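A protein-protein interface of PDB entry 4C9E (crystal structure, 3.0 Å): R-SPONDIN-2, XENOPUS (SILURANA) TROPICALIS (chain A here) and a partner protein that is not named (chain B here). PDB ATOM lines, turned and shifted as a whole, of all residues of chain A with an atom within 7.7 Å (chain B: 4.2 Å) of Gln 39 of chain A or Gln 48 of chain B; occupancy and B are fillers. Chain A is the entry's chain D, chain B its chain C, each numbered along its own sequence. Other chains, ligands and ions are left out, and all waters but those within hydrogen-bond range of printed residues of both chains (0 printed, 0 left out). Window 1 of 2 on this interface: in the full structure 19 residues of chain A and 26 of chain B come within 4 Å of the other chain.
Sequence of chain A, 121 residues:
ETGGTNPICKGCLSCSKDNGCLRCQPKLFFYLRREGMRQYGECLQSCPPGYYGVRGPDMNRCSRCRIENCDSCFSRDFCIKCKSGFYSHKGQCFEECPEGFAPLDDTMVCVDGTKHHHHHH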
ATOM      1  N   SER A  16     -17.575 -11.146  -7.106  1.00  0.00           N
ATOM      2  CA  SER A  16     -17.571 -12.575  -7.412  1.00  0.00           C
ATOM      3  C   SER A  16     -17.811 -13.405  -6.160  1.00  0.00           C
ATOM      4  O   SER A  16     -17.399 -13.034  -5.055  1.00  0.00           O
ATOM      5  CB  SER A  16     -16.262 -12.983  -8.069  1.00  0.00           C
ATOM      6  OG  SER A  16     -15.357 -13.521  -7.123  1.00  0.00           O
ATOM      7  N   LYS A  17     -18.477 -14.538  -6.348  1.00  0.00           N
ATOM      8  CA  LYS A  17     -18.813 -15.422  -5.245  1.00  0.00           C
ATOM      9  C   LYS A  17     -17.555 -15.998  -4.617  1.00  0.00           C
ATOM     10  O   LYS A  17     -17.539 -16.293  -3.434  1.00  0.00           O
ATOM     11  CB  LYS A  17     -19.766 -16.525  -5.715  1.00  0.00           C
ATOM     12  CG  LYS A  17     -21.179 -15.993  -5.931  1.00  0.00           C
ATOM     13  CD  LYS A  17     -22.005 -16.844  -6.882  1.00  0.00           C
ATOM     14  CE  LYS A  17     -23.355 -16.195  -7.162  1.00  0.00           C
ATOM     15  NZ  LYS A  17     -24.057 -16.834  -8.315  1.00  0.00           N
ATOM     16  N   ASP A  18     -16.491 -16.112  -5.403  1.00  0.00           N
ATOM     17  CA  ASP A  18     -15.244 -16.675  -4.908  1.00  0.00           C
ATOM     18  C   ASP A  18     -14.241 -15.671  -4.344  1.00  0.00           C
ATOM     19  O   ASP A  18     -13.531 -16.016  -3.406  1.00  0.00           O
ATOM     20  CB  ASP A  18     -14.589 -17.520  -6.000  1.00  0.00           C
ATOM     21  CG  ASP A  18     -15.313 -18.827  -6.223  1.00  0.00           C
ATOM     22  OD1 ASP A  18     -15.842 -19.373  -5.234  1.00  0.00           O
ATOM     23  OD2 ASP A  18     -15.354 -19.314  -7.372  1.00  0.00           O
ATOM     24  N   ASN A  19     -14.170 -14.458  -4.892  1.00  0.00           N
ATOM     25  CA  ASN A  19     -13.166 -13.466  -4.458  1.00  0.00           C
ATOM     26  C   ASN A  19     -13.720 -12.158  -3.897  1.00  0.00           C
ATOM     27  O   ASN A  19     -12.944 -11.256  -3.571  1.00  0.00           O
ATOM     28  CB  ASN A  19     -12.196 -13.131  -5.604  1.00  0.00           C
ATOM     29  CG  ASN A  19     -11.034 -14.117  -5.716  1.00  0.00           C
ATOM     30  OD1 ASN A  19     -10.569 -14.692  -4.722  1.00  0.00           O
ATOM     31  ND2 ASN A  19     -10.541 -14.300  -6.939  1.00  0.00           N
ATOM     32  N   GLY A  20     -15.040 -12.043  -3.771  1.00  0.00           N
ATOM     33  CA  GLY A  20     -15.645 -10.789  -3.320  1.00  0.00           C
ATOM     34  C   GLY A  20     -15.314  -9.661  -4.278  1.00  0.00           C
ATOM     35  O   GLY A  20     -15.287  -9.867  -5.493  1.00  0.00           O
ATOM     36  N   TYR A  31      -9.720  -3.445   0.054  1.00  0.00           N
ATOM     37  CA  TYR A  31      -9.132  -4.262   1.125  1.00  0.00           C
ATOM     38  C   TYR A  31      -9.362  -5.767   0.957  1.00  0.00           C
ATOM     39  O   TYR A  31     -10.419  -6.195   0.509  1.00  0.00           O
ATOM     40  CB  TYR A  31      -9.737  -3.844   2.442  1.00  0.00           C
ATOM     41  CG  TYR A  31      -9.258  -4.605   3.649  1.00  0.00           C
ATOM     42  CD1 TYR A  31      -7.947  -4.508   4.084  1.00  0.00           C
ATOM     43  CD2 TYR A  31     -10.138  -5.360   4.395  1.00  0.00           C
ATOM     44  CE1 TYR A  31      -7.522  -5.171   5.221  1.00  0.00           C
ATOM     45  CE2 TYR A  31      -9.730  -6.023   5.533  1.00  0.00           C
ATOM     46  CZ  TYR A  31      -8.425  -5.927   5.938  1.00  0.00           C
ATOM     47  OH  TYR A  31      -8.036  -6.601   7.063  1.00  0.00           O
ATOM     48  N   LEU A  32      -8.364  -6.558   1.343  1.00  0.00           N
ATOM     49  CA  LEU A  32      -8.467  -8.024   1.361  1.00  0.00           C
ATOM     50  C   LEU A  32      -8.810  -8.558   2.758  1.00  0.00           C
ATOM     51  O   LEU A  32      -8.067  -8.333   3.721  1.00  0.00           O
ATOM     52  CB  LEU A  32      -7.145  -8.631   0.934  1.00  0.00           C
ATOM     53  CG  LEU A  32      -6.649  -8.178  -0.425  1.00  0.00           C
ATOM     54  CD1 LEU A  32      -5.170  -8.493  -0.541  1.00  0.00           C
ATOM     55  CD2 LEU A  32      -7.427  -8.855  -1.540  1.00  0.00           C
ATOM     56  N   ARG A  33      -9.929  -9.268   2.875  1.00  0.00           N
ATOM     57  CA  ARG A  33     -10.260  -9.909   4.146  1.00  0.00           C
ATOM     58  C   ARG A  33      -9.770 -11.348   4.077  1.00  0.00           C
ATOM     59  O   ARG A  33     -10.063 -12.079   3.109  1.00  0.00           O
ATOM     60  CB  ARG A  33     -11.759  -9.850   4.465  1.00  0.00           C
ATOM     61  CG  ARG A  33     -12.093  -9.606   5.940  1.00  0.00           C
ATOM     62  CD  ARG A  33     -13.489  -9.013   6.062  1.00  0.00           C
ATOM     63  NE  ARG A  33     -14.162  -9.244   7.338  1.00  0.00           N
ATOM     64  CZ  ARG A  33     -14.655 -10.416   7.753  1.00  0.00           C
ATOM     65  NH1 ARG A  33     -14.532 -11.522   7.016  1.00  0.00           N
ATOM     66  NH2 ARG A  33     -15.260 -10.491   8.936  1.00  0.00           N
ATOM     67  N   ARG A  34      -8.987 -11.712   5.098  1.00  0.00           N
ATOM     68  CA  ARG A  34      -8.510 -13.043   5.286  1.00  0.00           C
ATOM     69  C   ARG A  34      -9.397 -13.642   6.344  1.00  0.00           C
ATOM     70  O   ARG A  34      -9.332 -13.254   7.489  1.00  0.00           O
ATOM     71  CB  ARG A  34      -7.056 -13.004   5.727  1.00  0.00           C
ATOM     72  CG  ARG A  34      -6.315 -14.330   5.722  1.00  0.00           C
ATOM     73  CD  ARG A  34      -6.388 -15.037   4.388  1.00  0.00           C
ATOM     74  NE  ARG A  34      -5.165 -14.969   3.623  1.00  0.00           N
ATOM     75  CZ  ARG A  34      -5.005 -15.589   2.459  1.00  0.00           C
ATOM     76  NH1 ARG A  34      -5.968 -16.342   1.951  1.00  0.00           N
ATOM     77  NH2 ARG A  34      -3.857 -15.477   1.804  1.00  0.00           N
ATOM     78  N   GLU A  35     -10.254 -14.560   5.943  1.00  0.00           N
ATOM     79  CA  GLU A  35     -11.212 -15.186   6.823  1.00  0.00           C
ATOM     80  C   GLU A  35     -10.960 -16.696   6.679  1.00  0.00           C
ATOM     81  O   GLU A  35     -11.500 -17.344   5.765  1.00  0.00           O
ATOM     82  CB  GLU A  35     -12.618 -14.801   6.366  1.00  0.00           C
ATOM     83  CG  GLU A  35     -13.755 -15.415   7.160  1.00  0.00           C
ATOM     84  CD  GLU A  35     -14.124 -14.604   8.383  1.00  0.00           C
ATOM     85  OE1 GLU A  35     -13.505 -13.533   8.616  1.00  0.00           O
ATOM     86  OE2 GLU A  35     -15.057 -15.025   9.112  1.00  0.00           O
ATOM     87  N   GLY A  36     -10.102 -17.246   7.543  1.00  0.00           N
ATOM     88  CA  GLY A  36      -9.655 -18.624   7.396  1.00  0.00           C
ATOM     89  C   GLY A  36      -8.759 -18.844   6.183  1.00  0.00           C
ATOM     90  O   GLY A  36      -7.733 -18.195   6.034  1.00  0.00           O
ATOM     91  N   MET A  37      -9.137 -19.760   5.303  1.00  0.00           N
ATOM     92  CA  MET A  37      -8.327 -20.003   4.118  1.00  0.00           C
ATOM     93  C   MET A  37      -8.620 -18.941   3.084  1.00  0.00           C
ATOM     94  O   MET A  37      -7.878 -18.794   2.112  1.00  0.00           O
ATOM     95  CB  MET A  37      -8.594 -21.362   3.490  1.00  0.00           C
ATOM     96  CG  MET A  37      -8.654 -22.497   4.496  1.00  0.00           C
ATOM     97  SD  MET A  37      -9.023 -24.130   3.459  1.00  0.00           S
ATOM     98  CE  MET A  37     -10.978 -24.086   3.570  1.00  0.00           C
ATOM     99  N   ARG A  38      -9.697 -18.183   3.285  1.00  0.00           N
ATOM    100  CA  ARG A  38     -10.224 -17.317   2.243  1.00  0.00           C
ATOM    101  C   ARG A  38      -9.577 -15.957   2.229  1.00  0.00           C
ATOM    102  O   ARG A  38      -9.208 -15.395   3.262  1.00  0.00           O
ATOM    103  CB  ARG A  38     -11.720 -17.117   2.407  1.00  0.00           C
ATOM    104  CG  ARG A  38     -12.523 -18.401   2.369  1.00  0.00           C
ATOM    105  CD  ARG A  38     -13.913 -18.139   2.890  1.00  0.00           C
ATOM    106  NE  ARG A  38     -14.565 -17.097   2.100  1.00  0.00           N
ATOM    107  CZ  ARG A  38     -15.543 -16.310   2.536  1.00  0.00           C
ATOM    108  NH1 ARG A  38     -16.009 -16.414   3.779  1.00  0.00           N
ATOM    109  NH2 ARG A  38     -16.056 -15.398   1.724  1.00  0.00           N
ATOM    110  N   GLN A  39      -9.441 -15.442   1.019  1.00  0.00           N
ATOM    111  CA  GLN A  39      -9.116 -14.058   0.832  1.00  0.00           C
ATOM    112  C   GLN A  39     -10.055 -13.542  -0.213  1.00  0.00           C
ATOM    113  O   GLN A  39     -10.145 -14.119  -1.290  1.00  0.00           O
ATOM    114  CB  GLN A  39      -7.688 -13.881   0.371  1.00  0.00           C
ATOM    115  CG  GLN A  39      -7.311 -12.426   0.401  1.00  0.00           C
ATOM    116  CD  GLN A  39      -5.829 -12.218   0.399  1.00  0.00           C
ATOM    117  OE1 GLN A  39      -5.154 -12.555  -0.579  1.00  0.00           O
ATOM    118  NE2 GLN A  39      -5.301 -11.645   1.494  1.00  0.00           N
ATOM    119  N   TYR A  40     -10.780 -12.480   0.132  1.00  0.00           N
ATOM    120  CA  TYR A  40     -11.767 -11.846  -0.762  1.00  0.00           C
ATOM    121  C   TYR A  40     -11.723 -10.341  -0.516  1.00  0.00           C
ATOM    122  O   TYR A  40     -11.259  -9.887   0.547  1.00  0.00           O
ATOM    123  CB  TYR A  40     -13.201 -12.413  -0.558  1.00  0.00           C
ATOM    124  CG  TYR A  40     -13.715 -12.352   0.871  1.00  0.00           C
ATOM    125  CD1 TYR A  40     -14.224 -11.176   1.394  1.00  0.00           C
ATOM    126  CD2 TYR A  40     -13.682 -13.471   1.702  1.00  0.00           C
ATOM    127  CE1 TYR A  40     -14.685 -11.106   2.703  1.00  0.00           C
ATOM    128  CE2 TYR A  40     -14.130 -13.407   3.015  1.00  0.00           C
ATOM    129  CZ  TYR A  40     -14.634 -12.222   3.506  1.00  0.00           C
ATOM    130  OH  TYR A  40     -15.088 -12.158   4.797  1.00  0.00           O
ATOM    131  N   GLY A  41     -12.207  -9.574  -1.491  1.00  0.00           N
ATOM    132  CA  GLY A  41     -12.119  -8.111  -1.438  1.00  0.00           C
ATOM    133  C   GLY A  41     -13.317  -7.424  -0.808  1.00  0.00           C
ATOM    134  O   GLY A  41     -14.451  -7.814  -1.056  1.00  0.00           O
ATOM    135  N   VAL B  47      -4.318 -22.088   1.289  1.00  0.00           N
ATOM    136  CA  VAL B  47      -4.518 -20.683   1.506  1.00  0.00           C
ATOM    137  C   VAL B  47      -5.001 -20.135   0.186  1.00  0.00           C
ATOM    138  O   VAL B  47      -4.356 -20.336  -0.827  1.00  0.00           O
ATOM    139  CB  VAL B  47      -3.203 -19.984   1.920  1.00  0.00           C
ATOM    140  CG1 VAL B  47      -3.386 -18.482   1.951  1.00  0.00           C
ATOM    141  CG2 VAL B  47      -2.737 -20.502   3.277  1.00  0.00           C
ATOM    142  N   GLN B  48      -6.147 -19.471   0.192  1.00  0.00           N
ATOM    143  CA  GLN B  48      -6.652 -18.855  -1.010  1.00  0.00           C
ATOM    144  C   GLN B  48      -5.876 -17.562  -1.192  1.00  0.00           C
ATOM    145  O   GLN B  48      -5.301 -17.041  -0.237  1.00  0.00           O
ATOM    146  CB  GLN B  48      -8.141 -18.547  -0.869  1.00  0.00           C
ATOM    147  CG  GLN B  48      -8.708 -17.657  -1.964  1.00  0.00           C
ATOM    148  CD  GLN B  48     -10.218 -17.642  -1.969  1.00  0.00           C
ATOM    149  OE1 GLN B  48     -10.859 -17.360  -0.952  1.00  0.00           O
ATOM    150  NE2 GLN B  48     -10.800 -17.942  -3.118  1.00  0.00           N
ATOM    151  N   MET B  49      -5.855 -17.038  -2.412  1.00  0.00           N
ATOM    152  CA  MET B  49      -5.308 -15.706  -2.647  1.00  0.00           C
ATOM    153  C   MET B  49      -6.184 -14.898  -3.640  1.00  0.00           C
ATOM    154  O   MET B  49      -6.712 -15.408  -4.639  1.00  0.00           O
ATOM    155  CB  MET B  49      -3.849 -15.810  -3.139  1.00  0.00           C
ATOM    156  CG  MET B  49      -2.834 -16.469  -2.197  1.00  0.00           C
ATOM    157  SD  MET B  49      -2.436 -15.624  -0.636  1.00  0.00           S
ATOM    158  CE  MET B  49      -1.784 -14.070  -1.203  1.00  0.00           C
ATOM    159  N   HIS B  50      -6.367 -13.627  -3.323  1.00  0.00           N
ATOM    160  CA  HIS B  50      -6.996 -12.703  -4.252  1.00  0.00           C
ATOM    161  C   HIS B  50      -5.947 -12.463  -5.329  1.00  0.00           C
ATOM    162  O   HIS B  50      -4.781 -12.235  -5.010  1.00  0.00           O
ATOM    163  CB  HIS B  50      -7.352 -11.393  -3.538  1.00  0.00           C
ATOM    164  CG  HIS B  50      -8.458 -10.628  -4.187  1.00  0.00           C
ATOM    165  ND1 HIS B  50      -8.511 -10.397  -5.545  1.00  0.00           N
ATOM    166  CD2 HIS B  50      -9.555 -10.035  -3.662  1.00  0.00           C
ATOM    167  CE1 HIS B  50      -9.592  -9.696  -5.829  1.00  0.00           C
ATOM    168  NE2 HIS B  50     -10.242  -9.458  -4.704  1.00  0.00           N
ATOM    169  N   TYR B  64       3.355 -15.204   5.759  1.00  0.00           N
ATOM    170  CA  TYR B  64       2.678 -16.484   5.860  1.00  0.00           C
ATOM    171  C   TYR B  64       3.688 -17.562   6.291  1.00  0.00           C
ATOM    172  O   TYR B  64       4.921 -17.418   6.125  1.00  0.00           O
ATOM    173  CB  TYR B  64       2.036 -16.869   4.500  1.00  0.00           C
ATOM    174  CG  TYR B  64       0.885 -15.986   4.031  1.00  0.00           C
ATOM    175  CD1 TYR B  64       0.201 -15.141   4.908  1.00  0.00           C
ATOM    176  CD2 TYR B  64       0.457 -16.028   2.710  1.00  0.00           C
ATOM    177  CE1 TYR B  64      -0.852 -14.351   4.472  1.00  0.00           C
ATOM    178  CE2 TYR B  64      -0.596 -15.242   2.264  1.00  0.00           C
ATOM    179  CZ  TYR B  64      -1.238 -14.406   3.149  1.00  0.00           C
ATOM    180  OH  TYR B  64      -2.279 -13.629   2.714  1.00  0.00           O
ATOM    181  N   VAL B  71      -4.290 -21.237  -3.613  1.00  0.00           N
ATOM    182  CA  VAL B  71      -5.350 -21.321  -4.586  1.00  0.00           C
ATOM    183  C   VAL B  71      -5.806 -19.930  -4.952  1.00  0.00           C
ATOM    184  O   VAL B  71      -6.181 -19.144  -4.069  1.00  0.00           O
ATOM    185  CB  VAL B  71      -6.615 -21.976  -4.064  1.00  0.00           C
ATOM    186  CG1 VAL B  71      -7.599 -22.017  -5.222  1.00  0.00           C
ATOM    187  CG2 VAL B  71      -6.336 -23.365  -3.471  1.00  0.00           C
ATOM    188  N   MET B 140     -13.115 -24.671  -5.207  1.00  0.00           N
ATOM    189  CA  MET B 140     -13.556 -23.411  -4.612  1.00  0.00           C
ATOM    190  C   MET B 140     -14.601 -23.626  -3.540  1.00  0.00           C
ATOM    191  O   MET B 140     -14.653 -22.876  -2.567  1.00  0.00           O
ATOM    192  CB  MET B 140     -14.160 -22.464  -5.651  1.00  0.00           C
ATOM    193  CG  MET B 140     -13.179 -21.650  -6.475  1.00  0.00           C
ATOM    194  SD  MET B 140     -11.724 -21.136  -5.561  1.00  0.00           S
ATOM    195  CE  MET B 140     -10.685 -22.518  -6.015  1.00  0.00           C
ATOM    196  N   VAL B 143     -12.846 -24.441  -0.212  1.00  0.00           N
ATOM    197  CA  VAL B 143     -12.206 -23.188   0.210  1.00  0.00           C
ATOM    198  C   VAL B 143     -13.165 -22.217   0.911  1.00  0.00           C
ATOM    199  O   VAL B 143     -12.893 -21.695   2.012  1.00  0.00           O
ATOM    200  CB  VAL B 143     -11.668 -22.452  -1.029  1.00  0.00           C
ATOM    201  CG1 VAL B 143     -11.143 -21.070  -0.660  1.00  0.00           C
ATOM    202  CG2 VAL B 143     -10.598 -23.279  -1.722  1.00  0.00           C
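NE2 of Gln 48 of chain B sits at hydrogen-bond distance from O of Asp 18 of chain A, 3.4 Å away. NH2 of Arg 34 of chain A lies within hydrogen-bond range of O of Gln 48 of chain B (2.9 Å). The backbone NH (N) of Gln 48 of chain B lies within hydrogen-bond range of the backbone carbonyl oxygen (O) of Met 37 of chain A (2.7 Å). The side-chain amide oxygen (OE1) of Gln 48 of chain B is in hydrogen-bond range of the backbone NH (N) of Gln 39 of chain A (3.1 Å). The side-chain sulfur (SD) of Met 49 of chain B sits at hydrogen-bond distance from the guanidinium group (NH2) of Arg 34 of chain A (2.8 Å). The backbone carbonyl oxygen (O) of Asn 19 of chain A sits at hydrogen-bond distance from a ring nitrogen (NE2) of His 50 of chain B, at 3.4 Å. The side-chain amide oxygen (OE1) of Gln 39 of chain A sits at hydrogen-bond distance from the backbone NH (N) of His 50 of chain B, at 3.2 Å. OH of Tyr 64 of chain B is in hydrogen-bond range of NH2 of Arg 34 of chain A (2.6 Å).
N of Val 71 of chain B lies within hydrogen-bond range of O of Val 47 of chain B, at 2.9 Å. N of Met 49 of chain B is in hydrogen-bond range of O of Val 71 of chain B, 2.7 Å away. OG of Ser 16 of chain A lies close to N of Asp 18 of chain A (3.3 Å). The backbone NH (N) of Asn 19 of chain A is in hydrogen-bond range of the side-chain hydroxyl (OG) of Ser 16 of chain A (2.7 Å). The backbone carbonyl oxygen (O) of Tyr 40 of chain A sits at hydrogen-bond distance from the backbone NH (N) of Arg 33 of chain A, at 2.8 Å. O of Met 37 of chain A is in hydrogen-bond range of NH1 of Arg 34 of chain A.
CG of Met 140 of chain B touches OD2 of Asp 18 of chain A, 3.3 Å away. Asn 19 of chain A touches Gln 48 of chain B (OD1 to NE2, 3.6 Å). Asn 19 of chain A touches Met 49 of chain B (OD1 to O, 3.9 Å). CD2 of His 50 of chain B touches CD2 of Leu 32 of chain A, 3.2 Å away. Val 47 of chain B touches Arg 34 of chain A. O of Val 143 of chain B touches CE of Met 37 of chain A, 3.4 Å away. Gln 48 of chain B touches Arg 38 of chain A (OE1 to CA, 3.3 Å). Arg 38 of chain A touches Val 143 of chain B (CG to O, 3.3 Å). Tyr 64 of chain B touches Gln 39 of chain A (OH to NE2, 3.8 Å). Tyr 40 of chain A touches His 50 of chain B (C to CD2, 3.8 Å).
Of the printed residues of chain B, Arg 34 of chain A touches Val 47, Gln 48, Met 49 and Tyr 64. Of the printed residues of chain B, Met 37 of chain A touches Val 47 (3.7 Å), Gln 48 (2.7 Å) and Val 143 (3.4 Å). Of the printed residues of chain A, Met 49 of chain B touches Asn 19 (3.9 Å), Arg 34 (2.8 Å) and Gln 39 (3.7 Å). Val 71 of chain B touches none of the printed residues of chain A. Printed residues of chain A within 4 Å of Met 140 of chain B: Asp 18. The nearest printed residue of chain B that does not touch Met 37 of chain A is Met 49 of chain B (5.3 Å).
Hydrophobic or aromatic side chains of chain A within 4 Å of the printed part of chain B: Leu 32 and Met 37. Of the 8 printed residues of chain B, 7 touch a printed residue of chain A. Printed residues of chain B that touch a printed residue of chain A: Val 47, Gln 48, Met 49, His 50, Tyr 64, Met 140 and Val 143. Hydrophobic or aromatic side chains of chain B within 4 Å of the printed part of chain A: Val 47, Met 49, His 50, Tyr 64 and Met 140. Among the printed residues, 21 pairs touch across the chains.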
